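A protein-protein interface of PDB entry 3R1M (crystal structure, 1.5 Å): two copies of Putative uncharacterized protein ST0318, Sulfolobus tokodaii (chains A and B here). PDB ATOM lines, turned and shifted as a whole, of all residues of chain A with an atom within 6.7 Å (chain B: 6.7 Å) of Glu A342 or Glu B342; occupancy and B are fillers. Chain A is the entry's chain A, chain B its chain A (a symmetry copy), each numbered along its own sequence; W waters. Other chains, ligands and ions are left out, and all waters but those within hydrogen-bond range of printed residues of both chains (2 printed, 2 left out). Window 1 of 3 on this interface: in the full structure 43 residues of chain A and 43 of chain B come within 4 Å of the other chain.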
ATOM      1  N   TYR A 174       6.199 -10.768  35.492  1.00  0.00           N
ATOM      2  CA  TYR A 174       5.075 -10.825  34.567  1.00  0.00           C
ATOM      3  C   TYR A 174       4.103 -11.916  35.007  1.00  0.00           C
ATOM      4  O   TYR A 174       2.887 -11.711  34.993  1.00  0.00           O
ATOM      5  CB  TYR A 174       5.538 -11.064  33.123  1.00  0.00           C
ATOM      6  CG  TYR A 174       6.336  -9.927  32.483  1.00  0.00           C
ATOM      7  CD1 TYR A 174       6.389  -8.659  33.054  1.00  0.00           C
ATOM      8  CD2 TYR A 174       7.006 -10.127  31.282  1.00  0.00           C
ATOM      9  CE1 TYR A 174       7.116  -7.621  32.447  1.00  0.00           C
ATOM     10  CE2 TYR A 174       7.720  -9.105  30.672  1.00  0.00           C
ATOM     11  CZ  TYR A 174       7.775  -7.859  31.262  1.00  0.00           C
ATOM     12  OH  TYR A 174       8.491  -6.854  30.639  1.00  0.00           O
ATOM     13  N   THR A 196      17.499 -10.353  31.590  1.00  0.00           N
ATOM     14  CA  THR A 196      16.297  -9.643  31.120  1.00  0.00           C
ATOM     15  C   THR A 196      15.628  -8.961  32.316  1.00  0.00           C
ATOM     16  O   THR A 196      14.683  -9.476  32.915  1.00  0.00           O
ATOM     17  CB  THR A 196      15.309 -10.602  30.418  1.00  0.00           C
ATOM     18  OG1 THR A 196      15.992 -11.332  29.404  1.00  0.00           O
ATOM     19  CG2 THR A 196      14.138  -9.847  29.827  1.00  0.00           C
ATOM     20  N   ALA A 198      13.720  -6.521  33.014  1.00  0.00           N
ATOM     21  CA  ALA A 198      12.353  -6.017  33.015  1.00  0.00           C
ATOM     22  C   ALA A 198      11.399  -7.126  33.418  1.00  0.00           C
ATOM     23  O   ALA A 198      10.278  -6.853  33.876  1.00  0.00           O
ATOM     24  CB  ALA A 198      11.983  -5.498  31.649  1.00  0.00           C
ATOM     25  N   PRO A 262      17.234   0.731  32.492  1.00  0.00           N
ATOM     26  CA  PRO A 262      16.079   1.282  31.783  1.00  0.00           C
ATOM     27  C   PRO A 262      15.346   2.315  32.622  1.00  0.00           C
ATOM     28  O   PRO A 262      15.254   2.163  33.849  1.00  0.00           O
ATOM     29  CB  PRO A 262      15.189   0.050  31.571  1.00  0.00           C
ATOM     30  CG  PRO A 262      15.510  -0.840  32.717  1.00  0.00           C
ATOM     31  CD  PRO A 262      16.976  -0.613  33.038  1.00  0.00           C
ATOM     32  N   SER A 268      11.473   5.666  29.025  1.00  0.00           N
ATOM     33  CA  SER A 268      11.554   5.079  27.694  1.00  0.00           C
ATOM     34  C   SER A 268      12.975   4.890  27.185  1.00  0.00           C
ATOM     35  O   SER A 268      13.165   4.642  26.002  1.00  0.00           O
ATOM     36  CB  SER A 268      10.805   5.951  26.684  1.00  0.00           C
ATOM     37  OG  SER A 268       9.421   5.924  26.957  1.00  0.00           O
ATOM     38  N   TYR A 270      17.435   3.687  27.892  1.00  0.00           N
ATOM     39  CA  TYR A 270      18.570   3.204  28.690  1.00  0.00           C
ATOM     40  C   TYR A 270      19.574   4.320  28.905  1.00  0.00           C
ATOM     41  O   TYR A 270      19.909   5.053  27.989  1.00  0.00           O
ATOM     42  CB  TYR A 270      19.249   2.048  27.972  1.00  0.00           C
ATOM     43  CG  TYR A 270      18.472   0.767  28.051  1.00  0.00           C
ATOM     44  CD1 TYR A 270      18.562  -0.046  29.161  1.00  0.00           C
ATOM     45  CD2 TYR A 270      17.633   0.398  27.005  1.00  0.00           C
ATOM     46  CE1 TYR A 270      17.852  -1.247  29.217  1.00  0.00           C
ATOM     47  CE2 TYR A 270      16.917  -0.770  27.050  1.00  0.00           C
ATOM     48  CZ  TYR A 270      17.021  -1.577  28.160  1.00  0.00           C
ATOM     49  OH  TYR A 270      16.289  -2.746  28.196  1.00  0.00           O
ATOM     50  N   MET A 337      16.410   2.506  19.281  1.00  0.00           N
ATOM     51  CA  MET A 337      16.972   1.412  20.069  1.00  0.00           C
ATOM     52  C   MET A 337      18.440   1.300  19.688  1.00  0.00           C
ATOM     53  O   MET A 337      18.792   1.576  18.548  1.00  0.00           O
ATOM     54  CB  MET A 337      16.247   0.094  19.747  1.00  0.00           C
ATOM     55  CG  MET A 337      14.805   0.114  20.226  1.00  0.00           C
ATOM     56  SD  MET A 337      13.980  -1.444  19.822  1.00  0.00           S
ATOM     57  CE  MET A 337      15.023  -2.609  20.691  1.00  0.00           C
ATOM     58  N   PRO A 338      19.309   0.936  20.639  1.00  0.00           N
ATOM     59  CA  PRO A 338      18.971   0.527  22.000  1.00  0.00           C
ATOM     60  C   PRO A 338      19.009   1.660  23.047  1.00  0.00           C
ATOM     61  O   PRO A 338      18.959   1.364  24.253  1.00  0.00           O
ATOM     62  CB  PRO A 338      20.060  -0.507  22.318  1.00  0.00           C
ATOM     63  CG  PRO A 338      21.298   0.102  21.649  1.00  0.00           C
ATOM     64  CD  PRO A 338      20.749   0.719  20.347  1.00  0.00           C
ATOM     65  N   ARG A 340      16.493   4.039  23.076  1.00  0.00           N
ATOM     66  CA  ARG A 340      15.066   3.884  23.363  1.00  0.00           C
ATOM     67  C   ARG A 340      14.822   2.437  23.759  1.00  0.00           C
ATOM     68  O   ARG A 340      15.489   1.532  23.272  1.00  0.00           O
ATOM     69  CB  ARG A 340      14.230   4.219  22.130  1.00  0.00           C
ATOM     70  CG  ARG A 340      12.773   4.539  22.449  1.00  0.00           C
ATOM     71  CD  ARG A 340      11.889   4.196  21.265  1.00  0.00           C
ATOM     72  NE  ARG A 340      11.774   2.749  21.232  1.00  0.00           N
ATOM     73  CZ  ARG A 340      11.354   2.028  20.185  1.00  0.00           C
ATOM     74  NH1 ARG A 340      11.273   0.709  20.291  1.00  0.00           N
ATOM     75  NH2 ARG A 340      11.052   2.618  19.031  1.00  0.00           N
ATOM     76  N   LEU A 341      13.836   2.238  24.641  1.00  0.00           N
ATOM     77  CA  LEU A 341      13.522   0.871  25.098  1.00  0.00           C
ATOM     78  C   LEU A 341      12.957  -0.017  24.006  1.00  0.00           C
ATOM     79  O   LEU A 341      12.346   0.447  23.014  1.00  0.00           O
ATOM     80  CB  LEU A 341      12.504   0.870  26.249  1.00  0.00           C
ATOM     81  CG  LEU A 341      12.920   1.517  27.549  1.00  0.00           C
ATOM     82  CD1 LEU A 341      11.949   1.110  28.681  1.00  0.00           C
ATOM     83  CD2 LEU A 341      14.356   1.164  27.883  1.00  0.00           C
ATOM     84  N   GLU A 342      13.148  -1.313  24.219  1.00  0.00           N
ATOM     85  CA  GLU A 342      12.576  -2.376  23.387  1.00  0.00           C
ATOM     86  C   GLU A 342      11.050  -2.325  23.364  1.00  0.00           C
ATOM     87  O   GLU A 342      10.408  -1.828  24.297  1.00  0.00           O
ATOM     88  CB  GLU A 342      13.101  -3.748  23.862  1.00  0.00           C
ATOM     89  CG  GLU A 342      12.618  -4.185  25.275  1.00  0.00           C
ATOM     90  CD  GLU A 342      13.375  -3.564  26.453  1.00  0.00           C
ATOM     91  OE1 GLU A 342      14.355  -2.815  26.252  1.00  0.00           O
ATOM     92  OE2 GLU A 342      12.979  -3.838  27.612  1.00  0.00           O
ATOM     93  N   PRO A 343      10.455  -2.834  22.279  1.00  0.00           N
ATOM     94  CA  PRO A 343       9.013  -2.680  22.079  1.00  0.00           C
ATOM     95  C   PRO A 343       8.177  -3.260  23.221  1.00  0.00           C
ATOM     96  O   PRO A 343       7.184  -2.660  23.592  1.00  0.00           O
ATOM     97  CB  PRO A 343       8.732  -3.446  20.772  1.00  0.00           C
ATOM     98  CG  PRO A 343      10.027  -3.860  20.227  1.00  0.00           C
ATOM     99  CD  PRO A 343      11.129  -3.561  21.187  1.00  0.00           C
ATOM    100  N   THR A 344       8.560  -4.404  23.775  1.00  0.00           N
ATOM    101  CA  THR A 344       7.723  -5.004  24.827  1.00  0.00           C
ATOM    102  C   THR A 344       7.575  -4.120  26.080  1.00  0.00           C
ATOM    103  O   THR A 344       6.567  -4.192  26.801  1.00  0.00           O
ATOM    104  CB  THR A 344       8.171  -6.434  25.176  1.00  0.00           C
ATOM    105  OG1 THR A 344       9.545  -6.426  25.587  1.00  0.00           O
ATOM    106  CG2 THR A 344       8.031  -7.314  23.968  1.00  0.00           C
ATOM    107  N   GLU A 345       8.546  -3.239  26.305  1.00  0.00           N
ATOM    108  CA  GLU A 345       8.485  -2.312  27.425  1.00  0.00           C
ATOM    109  C   GLU A 345       7.957  -0.925  27.020  1.00  0.00           C
ATOM    110  O   GLU A 345       7.410  -0.197  27.853  1.00  0.00           O
ATOM    111  CB  GLU A 345       9.856  -2.229  28.123  1.00  0.00           C
ATOM    112  CG  GLU A 345      10.156  -3.443  28.989  1.00  0.00           C
ATOM    113  CD  GLU A 345       9.165  -3.592  30.129  1.00  0.00           C
ATOM    114  OE1 GLU A 345       9.058  -2.672  30.976  1.00  0.00           O
ATOM    115  OE2 GLU A 345       8.508  -4.647  30.175  1.00  0.00           O
ATOM    116  N   MET A 346       8.077  -0.564  25.744  1.00  0.00           N
ATOM    117  CA  MET A 346       7.473   0.678  25.239  1.00  0.00           C
ATOM    118  C   MET A 346       5.967   0.542  25.176  1.00  0.00           C
ATOM    119  O   MET A 346       5.239   1.528  25.038  1.00  0.00           O
ATOM    120  CB  MET A 346       7.925   0.993  23.807  1.00  0.00           C
ATOM    121  CG  MET A 346       9.332   1.523  23.637  1.00  0.00           C
ATOM    122  SD  MET A 346       9.726   2.928  24.677  1.00  0.00           S
ATOM    123  CE  MET A 346       8.929   4.323  23.915  1.00  0.00           C
ATOM    124  N   GLU A 347       5.500  -0.695  25.219  1.00  0.00           N
ATOM    125  CA  GLU A 347       4.091  -0.937  25.000  1.00  0.00           C
ATOM    126  C   GLU A 347       3.259  -0.308  26.111  1.00  0.00           C
ATOM    127  O   GLU A 347       2.061  -0.078  25.934  1.00  0.00           O
ATOM    128  CB  GLU A 347       3.804  -2.433  24.864  1.00  0.00           C
ATOM    129  CG  GLU A 347       2.587  -2.713  24.011  1.00  0.00           C
ATOM    130  CD  GLU A 347       2.196  -4.168  24.039  1.00  0.00           C
ATOM    131  OE1 GLU A 347       1.792  -4.693  22.976  1.00  0.00           O
ATOM    132  OE2 GLU A 347       2.303  -4.789  25.123  1.00  0.00           O
ATOM    133  N   TYR B 174       8.179  -8.027   9.775  1.00  0.00           N
ATOM    134  CA  TYR B 174       7.451  -9.102  10.437  1.00  0.00           C
ATOM    135  C   TYR B 174       6.161  -9.393   9.676  1.00  0.00           C
ATOM    136  O   TYR B 174       5.808 -10.556   9.467  1.00  0.00           O
ATOM    137  CB  TYR B 174       7.148  -8.764  11.904  1.00  0.00           C
ATOM    138  CG  TYR B 174       8.363  -8.673  12.829  1.00  0.00           C
ATOM    139  CD1 TYR B 174       9.614  -9.143  12.444  1.00  0.00           C
ATOM    140  CD2 TYR B 174       8.233  -8.142  14.108  1.00  0.00           C
ATOM    141  CE1 TYR B 174      10.717  -9.064  13.312  1.00  0.00           C
ATOM    142  CE2 TYR B 174       9.317  -8.067  14.973  1.00  0.00           C
ATOM    143  CZ  TYR B 174      10.554  -8.523  14.567  1.00  0.00           C
ATOM    144  OH  TYR B 174      11.619  -8.440  15.443  1.00  0.00           O
ATOM    145  N   THR B 196      12.667   1.202  15.921  1.00  0.00           N
ATOM    146  CA  THR B 196      12.671  -0.241  16.221  1.00  0.00           C
ATOM    147  C   THR B 196      13.221  -0.994  15.008  1.00  0.00           C
ATOM    148  O   THR B 196      12.481  -1.510  14.169  1.00  0.00           O
ATOM    149  CB  THR B 196      11.257  -0.749  16.581  1.00  0.00           C
ATOM    150  OG1 THR B 196      10.708   0.062  17.614  1.00  0.00           O
ATOM    151  CG2 THR B 196      11.289  -2.200  17.011  1.00  0.00           C
ATOM    152  N   ALA B 198      14.672  -3.714  14.245  1.00  0.00           N
ATOM    153  CA  ALA B 198      14.519  -5.146  14.028  1.00  0.00           C
ATOM    154  C   ALA B 198      13.214  -5.417  13.304  1.00  0.00           C
ATOM    155  O   ALA B 198      13.058  -6.470  12.664  1.00  0.00           O
ATOM    156  CB  ALA B 198      14.535  -5.882  15.343  1.00  0.00           C
ATOM    157  N   PRO B 262      22.455  -4.067  16.372  1.00  0.00           N
ATOM    158  CA  PRO B 262      22.290  -5.423  16.893  1.00  0.00           C
ATOM    159  C   PRO B 262      23.048  -6.441  16.058  1.00  0.00           C
ATOM    160  O   PRO B 262      23.125  -6.299  14.829  1.00  0.00           O
ATOM    161  CB  PRO B 262      20.779  -5.658  16.764  1.00  0.00           C
ATOM    162  CG  PRO B 262      20.373  -4.820  15.606  1.00  0.00           C
ATOM    163  CD  PRO B 262      21.276  -3.600  15.622  1.00  0.00           C
ATOM    164  N   SER B 268      23.566 -11.842  19.178  1.00  0.00           N
ATOM    165  CA  SER B 268      22.815 -11.664  20.414  1.00  0.00           C
ATOM    166  C   SER B 268      23.164 -10.394  21.175  1.00  0.00           C
ATOM    167  O   SER B 268      22.788 -10.259  22.331  1.00  0.00           O
ATOM    168  CB  SER B 268      23.048 -12.851  21.351  1.00  0.00           C
ATOM    169  OG  SER B 268      22.476 -14.018  20.800  1.00  0.00           O
ATOM    170  N   TYR B 270      24.195  -5.836  21.248  1.00  0.00           N
ATOM    171  CA  TYR B 270      24.430  -4.517  20.645  1.00  0.00           C
ATOM    172  C   TYR B 270      25.889  -4.128  20.780  1.00  0.00           C
ATOM    173  O   TYR B 270      26.491  -4.289  21.829  1.00  0.00           O
ATOM    174  CB  TYR B 270      23.566  -3.474  21.336  1.00  0.00           C
ATOM    175  CG  TYR B 270      22.120  -3.551  20.942  1.00  0.00           C
ATOM    176  CD1 TYR B 270      21.672  -2.956  19.781  1.00  0.00           C
ATOM    177  CD2 TYR B 270      21.217  -4.245  21.740  1.00  0.00           C
ATOM    178  CE1 TYR B 270      20.322  -3.013  19.431  1.00  0.00           C
ATOM    179  CE2 TYR B 270      19.891  -4.325  21.404  1.00  0.00           C
ATOM    180  CZ  TYR B 270      19.455  -3.721  20.247  1.00  0.00           C
ATOM    181  OH  TYR B 270      18.118  -3.815  19.917  1.00  0.00           O
ATOM    182  N   MET B 337      20.957  -7.259  29.253  1.00  0.00           N
ATOM    183  CA  MET B 337      20.404  -6.160  28.466  1.00  0.00           C
ATOM    184  C   MET B 337      20.867  -4.868  29.122  1.00  0.00           C
ATOM    185  O   MET B 337      21.030  -4.830  30.335  1.00  0.00           O
ATOM    186  CB  MET B 337      18.867  -6.224  28.467  1.00  0.00           C
ATOM    187  CG  MET B 337      18.354  -7.438  27.710  1.00  0.00           C
ATOM    188  SD  MET B 337      16.547  -7.488  27.741  1.00  0.00           S
ATOM    189  CE  MET B 337      16.156  -5.924  26.964  1.00  0.00           C
ATOM    190  N   PRO B 338      21.120  -3.819  28.330  1.00  0.00           N
ATOM    191  CA  PRO B 338      20.892  -3.756  26.888  1.00  0.00           C
ATOM    192  C   PRO B 338      22.116  -4.118  26.021  1.00  0.00           C
ATOM    193  O   PRO B 338      22.080  -3.874  24.803  1.00  0.00           O
ATOM    194  CB  PRO B 338      20.525  -2.281  26.673  1.00  0.00           C
ATOM    195  CG  PRO B 338      21.461  -1.562  27.652  1.00  0.00           C
ATOM    196  CD  PRO B 338      21.498  -2.492  28.880  1.00  0.00           C
ATOM    197  N   ARG B 340      23.112  -7.425  25.776  1.00  0.00           N
ATOM    198  CA  ARG B 340      22.413  -8.569  25.187  1.00  0.00           C
ATOM    199  C   ARG B 340      21.119  -8.062  24.573  1.00  0.00           C
ATOM    200  O   ARG B 340      20.516  -7.117  25.068  1.00  0.00           O
ATOM    201  CB  ARG B 340      22.092  -9.611  26.255  1.00  0.00           C
ATOM    202  CG  ARG B 340      21.802 -10.998  25.688  1.00  0.00           C
ATOM    203  CD  ARG B 340      20.875 -11.761  26.615  1.00  0.00           C
ATOM    204  NE  ARG B 340      19.550 -11.194  26.443  1.00  0.00           N
ATOM    205  CZ  ARG B 340      18.521 -11.358  27.285  1.00  0.00           C
ATOM    206  NH1 ARG B 340      17.351 -10.803  27.001  1.00  0.00           N
ATOM    207  NH2 ARG B 340      18.672 -12.040  28.417  1.00  0.00           N
ATOM    208  N   LEU B 341      20.695  -8.724  23.490  1.00  0.00           N
ATOM    209  CA  LEU B 341      19.453  -8.307  22.812  1.00  0.00           C
ATOM    210  C   LEU B 341      18.205  -8.526  23.647  1.00  0.00           C
ATOM    211  O   LEU B 341      18.144  -9.401  24.543  1.00  0.00           O
ATOM    212  CB  LEU B 341      19.244  -9.056  21.487  1.00  0.00           C
ATOM    213  CG  LEU B 341      20.257  -8.830  20.390  1.00  0.00           C
ATOM    214  CD1 LEU B 341      19.708  -9.351  19.042  1.00  0.00           C
ATOM    215  CD2 LEU B 341      20.641  -7.365  20.315  1.00  0.00           C
ATOM    216  N   GLU B 342      17.196  -7.730  23.317  1.00  0.00           N
ATOM    217  CA  GLU B 342      15.845  -7.842  23.876  1.00  0.00           C
ATOM    218  C   GLU B 342      15.221  -9.206  23.593  1.00  0.00           C
ATOM    219  O   GLU B 342      15.568  -9.883  22.618  1.00  0.00           O
ATOM    220  CB  GLU B 342      14.968  -6.685  23.351  1.00  0.00           C
ATOM    221  CG  GLU B 342      14.663  -6.729  21.826  1.00  0.00           C
ATOM    222  CD  GLU B 342      15.776  -6.207  20.913  1.00  0.00           C
ATOM    223  OE1 GLU B 342      16.819  -5.721  21.403  1.00  0.00           O
ATOM    224  OE2 GLU B 342      15.600  -6.283  19.673  1.00  0.00           O
ATOM    225  N   PRO B 343      14.294  -9.627  24.462  1.00  0.00           N
ATOM    226  CA  PRO B 343      13.761 -10.988  24.381  1.00  0.00           C
ATOM    227  C   PRO B 343      13.120 -11.308  23.030  1.00  0.00           C
ATOM    228  O   PRO B 343      13.290 -12.412  22.542  1.00  0.00           O
ATOM    229  CB  PRO B 343      12.700 -11.041  25.497  1.00  0.00           C
ATOM    230  CG  PRO B 343      12.789  -9.781  26.239  1.00  0.00           C
ATOM    231  CD  PRO B 343      13.727  -8.834  25.569  1.00  0.00           C
ATOM    232  N   THR B 344      12.397 -10.373  22.427  1.00  0.00           N
ATOM    233  CA  THR B 344      11.722 -10.697  21.160  1.00  0.00           C
ATOM    234  C   THR B 344      12.687 -11.081  20.023  1.00  0.00           C
ATOM    235  O   THR B 344      12.332 -11.842  19.108  1.00  0.00           O
ATOM    236  CB  THR B 344      10.734  -9.596  20.735  1.00  0.00           C
ATOM    237  OG1 THR B 344      11.423  -8.345  20.617  1.00  0.00           O
ATOM    238  CG2 THR B 344       9.655  -9.461  21.769  1.00  0.00           C
ATOM    239  N   GLU B 345      13.928 -10.611  20.113  1.00  0.00           N
ATOM    240  CA  GLU B 345      14.944 -10.955  19.128  1.00  0.00           C
ATOM    241  C   GLU B 345      15.847 -12.113  19.587  1.00  0.00           C
ATOM    242  O   GLU B 345      16.417 -12.827  18.757  1.00  0.00           O
ATOM    243  CB  GLU B 345      15.755  -9.704  18.740  1.00  0.00           C
ATOM    244  CG  GLU B 345      14.998  -8.770  17.810  1.00  0.00           C
ATOM    245  CD  GLU B 345      14.669  -9.427  16.483  1.00  0.00           C
ATOM    246  OE1 GLU B 345      15.602  -9.843  15.752  1.00  0.00           O
ATOM    247  OE2 GLU B 345      13.467  -9.508  16.172  1.00  0.00           O
ATOM    248  N   MET B 346      15.956 -12.335  20.896  1.00  0.00           N
ATOM    249  CA  MET B 346      16.678 -13.504  21.417  1.00  0.00           C
ATOM    250  C   MET B 346      15.890 -14.769  21.154  1.00  0.00           C
ATOM    251  O   MET B 346      16.410 -15.883  21.263  1.00  0.00           O
ATOM    252  CB  MET B 346      16.859 -13.432  22.939  1.00  0.00           C
ATOM    253  CG  MET B 346      17.902 -12.466  23.457  1.00  0.00           C
ATOM    254  SD  MET B 346      19.517 -12.643  22.703  1.00  0.00           S
ATOM    255  CE  MET B 346      20.238 -14.085  23.454  1.00  0.00           C
ATOM    256  N   GLU B 347      14.611 -14.598  20.863  1.00  0.00           N
ATOM    257  CA  GLU B 347      13.741 -15.749  20.758  1.00  0.00           C
ATOM    258  C   GLU B 347      14.157 -16.632  19.588  1.00  0.00           C
ATOM    259  O   GLU B 347      13.801 -17.811  19.544  1.00  0.00           O
ATOM    260  CB  GLU B 347      12.277 -15.322  20.645  1.00  0.00           C
ATOM    261  CG  GLU B 347      11.327 -16.366  21.190  1.00  0.00           C
ATOM    262  CD  GLU B 347       9.886 -16.030  20.903  1.00  0.00           C
ATOM    263  OE1 GLU B 347       9.033 -16.272  21.786  1.00  0.00           O
ATOM    264  OE2 GLU B 347       9.610 -15.512  19.794  1.00  0.00           O
HETATM  265  O   HOH W   1      14.649  -6.386  30.158  1.00  0.00           O
HETATM  266  O   HOH W   2      14.614  -3.318  17.224  1.00  0.00           O
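NH1 of Arg A340 sits at hydrogen-bond distance from OG1 of Thr B196.
The guanidinium group (NH1) of Arg B340 lies within hydrogen-bond range of the side-chain hydroxyl (OG1) of Thr A196, at 2.8 Å.
The side-chain sulfur of Met B337 sits at hydrogen-bond distance from the guanidinium group of Arg B340, 3.5 Å away.
OE1 of Glu B342 sits at hydrogen-bond distance from OH of Tyr B270, at 2.7 Å.
The side-chain hydroxyl (OH) of Tyr A270 lies within hydrogen-bond range of the side-chain carboxylate (OE1) of Glu A342.
The guanidinium group (NH1) of Arg A340 lies within hydrogen-bond range of the side-chain sulfur (SD) of Met A337 (3.5 Å).
Among the printed residues, pairs that only touch across the chains: Thr A196 with Met B337 (3.96 Å), Thr A196 with Pro B343 (3.8 Å), Tyr A270 with Met B337 (3.4 Å), Tyr A270 with Pro B338 (3.6 Å), Met A337 with Thr B196 (3.96 Å), Met A337 with Tyr B270 (3.4 Å), Met A337 with Glu B342 (3.7 Å), Pro A338 with Tyr B270 (3.6 Å), Glu A342 with Met B337 (3.7 Å), Glu A342 with Glu B342 (3.5 Å), Pro A343 with Thr B196 (3.8 Å) and Thr A344 with Thr B344 (3.5 Å).
Glu A342 touches just these residues of chain B: Met B337 and Glu B342.
Glu B342 touches two residues of chain A.
Printed residues of chain B within 4 Å of Met A337: Thr B196, Tyr B270 and Glu B342.
Of the printed residues of chain A, Arg B340 touches Thr A196.
Of the printed residues of chain B, Tyr A270 touches Met B337 and Pro B338.
Of the printed residues of chain B, Arg A340 touches Thr B196 (2.8 Å).
Printed residues of chain A within 4 Å of Tyr B270: Met A337 (3.4 Å) and Pro A338 (3.6 Å).
Leu B341 touches none of the printed residues of chain A.
Glu A345 touches none of the printed residues of chain B.
Printed residues of chain B that touch a printed residue of chain A: Thr B196, Tyr B270, Met B337, Pro B338, Arg B340, Glu B342, Pro B343 and Thr B344.
Hydrophobic or aromatic side chains of chain B within 4 Å of the printed part of chain A: Tyr B270, Met B337, Pro B338 and Pro B343.
Among the printed residues, 14 pairs touch across the chains.
Among the printed residues, no Asp or Glu carboxylate lies within 4 Å of a Lys or Arg side-chain nitrogen of the other chain.
Thr A196 touches Met B337, and with the chains exchanged Met A337 touches Thr B196.
Thr A196 touches Arg B340, and with the chains exchanged Arg A340 touches Thr B196.
Tyr A270 touches Pro B338, and with the chains exchanged Pro A338 touches Tyr B270.
Met A337 touches Glu B342, and with the chains exchanged Glu A342 touches Met B337.
Positions printed for both chains: 174, 196, 198, 262, 268, 270, 337, 338, 340, 341, 342, 343, 344, 345, 346 and 347.
Of the 14 pairs that touch across the chains among the printed residues, 14 have their exchanged pair printed and touching as well.
Water W1 bridges the backbone NH (N) of Ala A198 (3.0 Å) and the side-chain sulfur (SD) of Met B337 (3.3 Å).
Water W2 lies within hydrogen-bond range of the backbone NH (N) of Ala B198 (3.0 Å) and the side-chain sulfur (SD) of Met A337 (3.3 Å).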
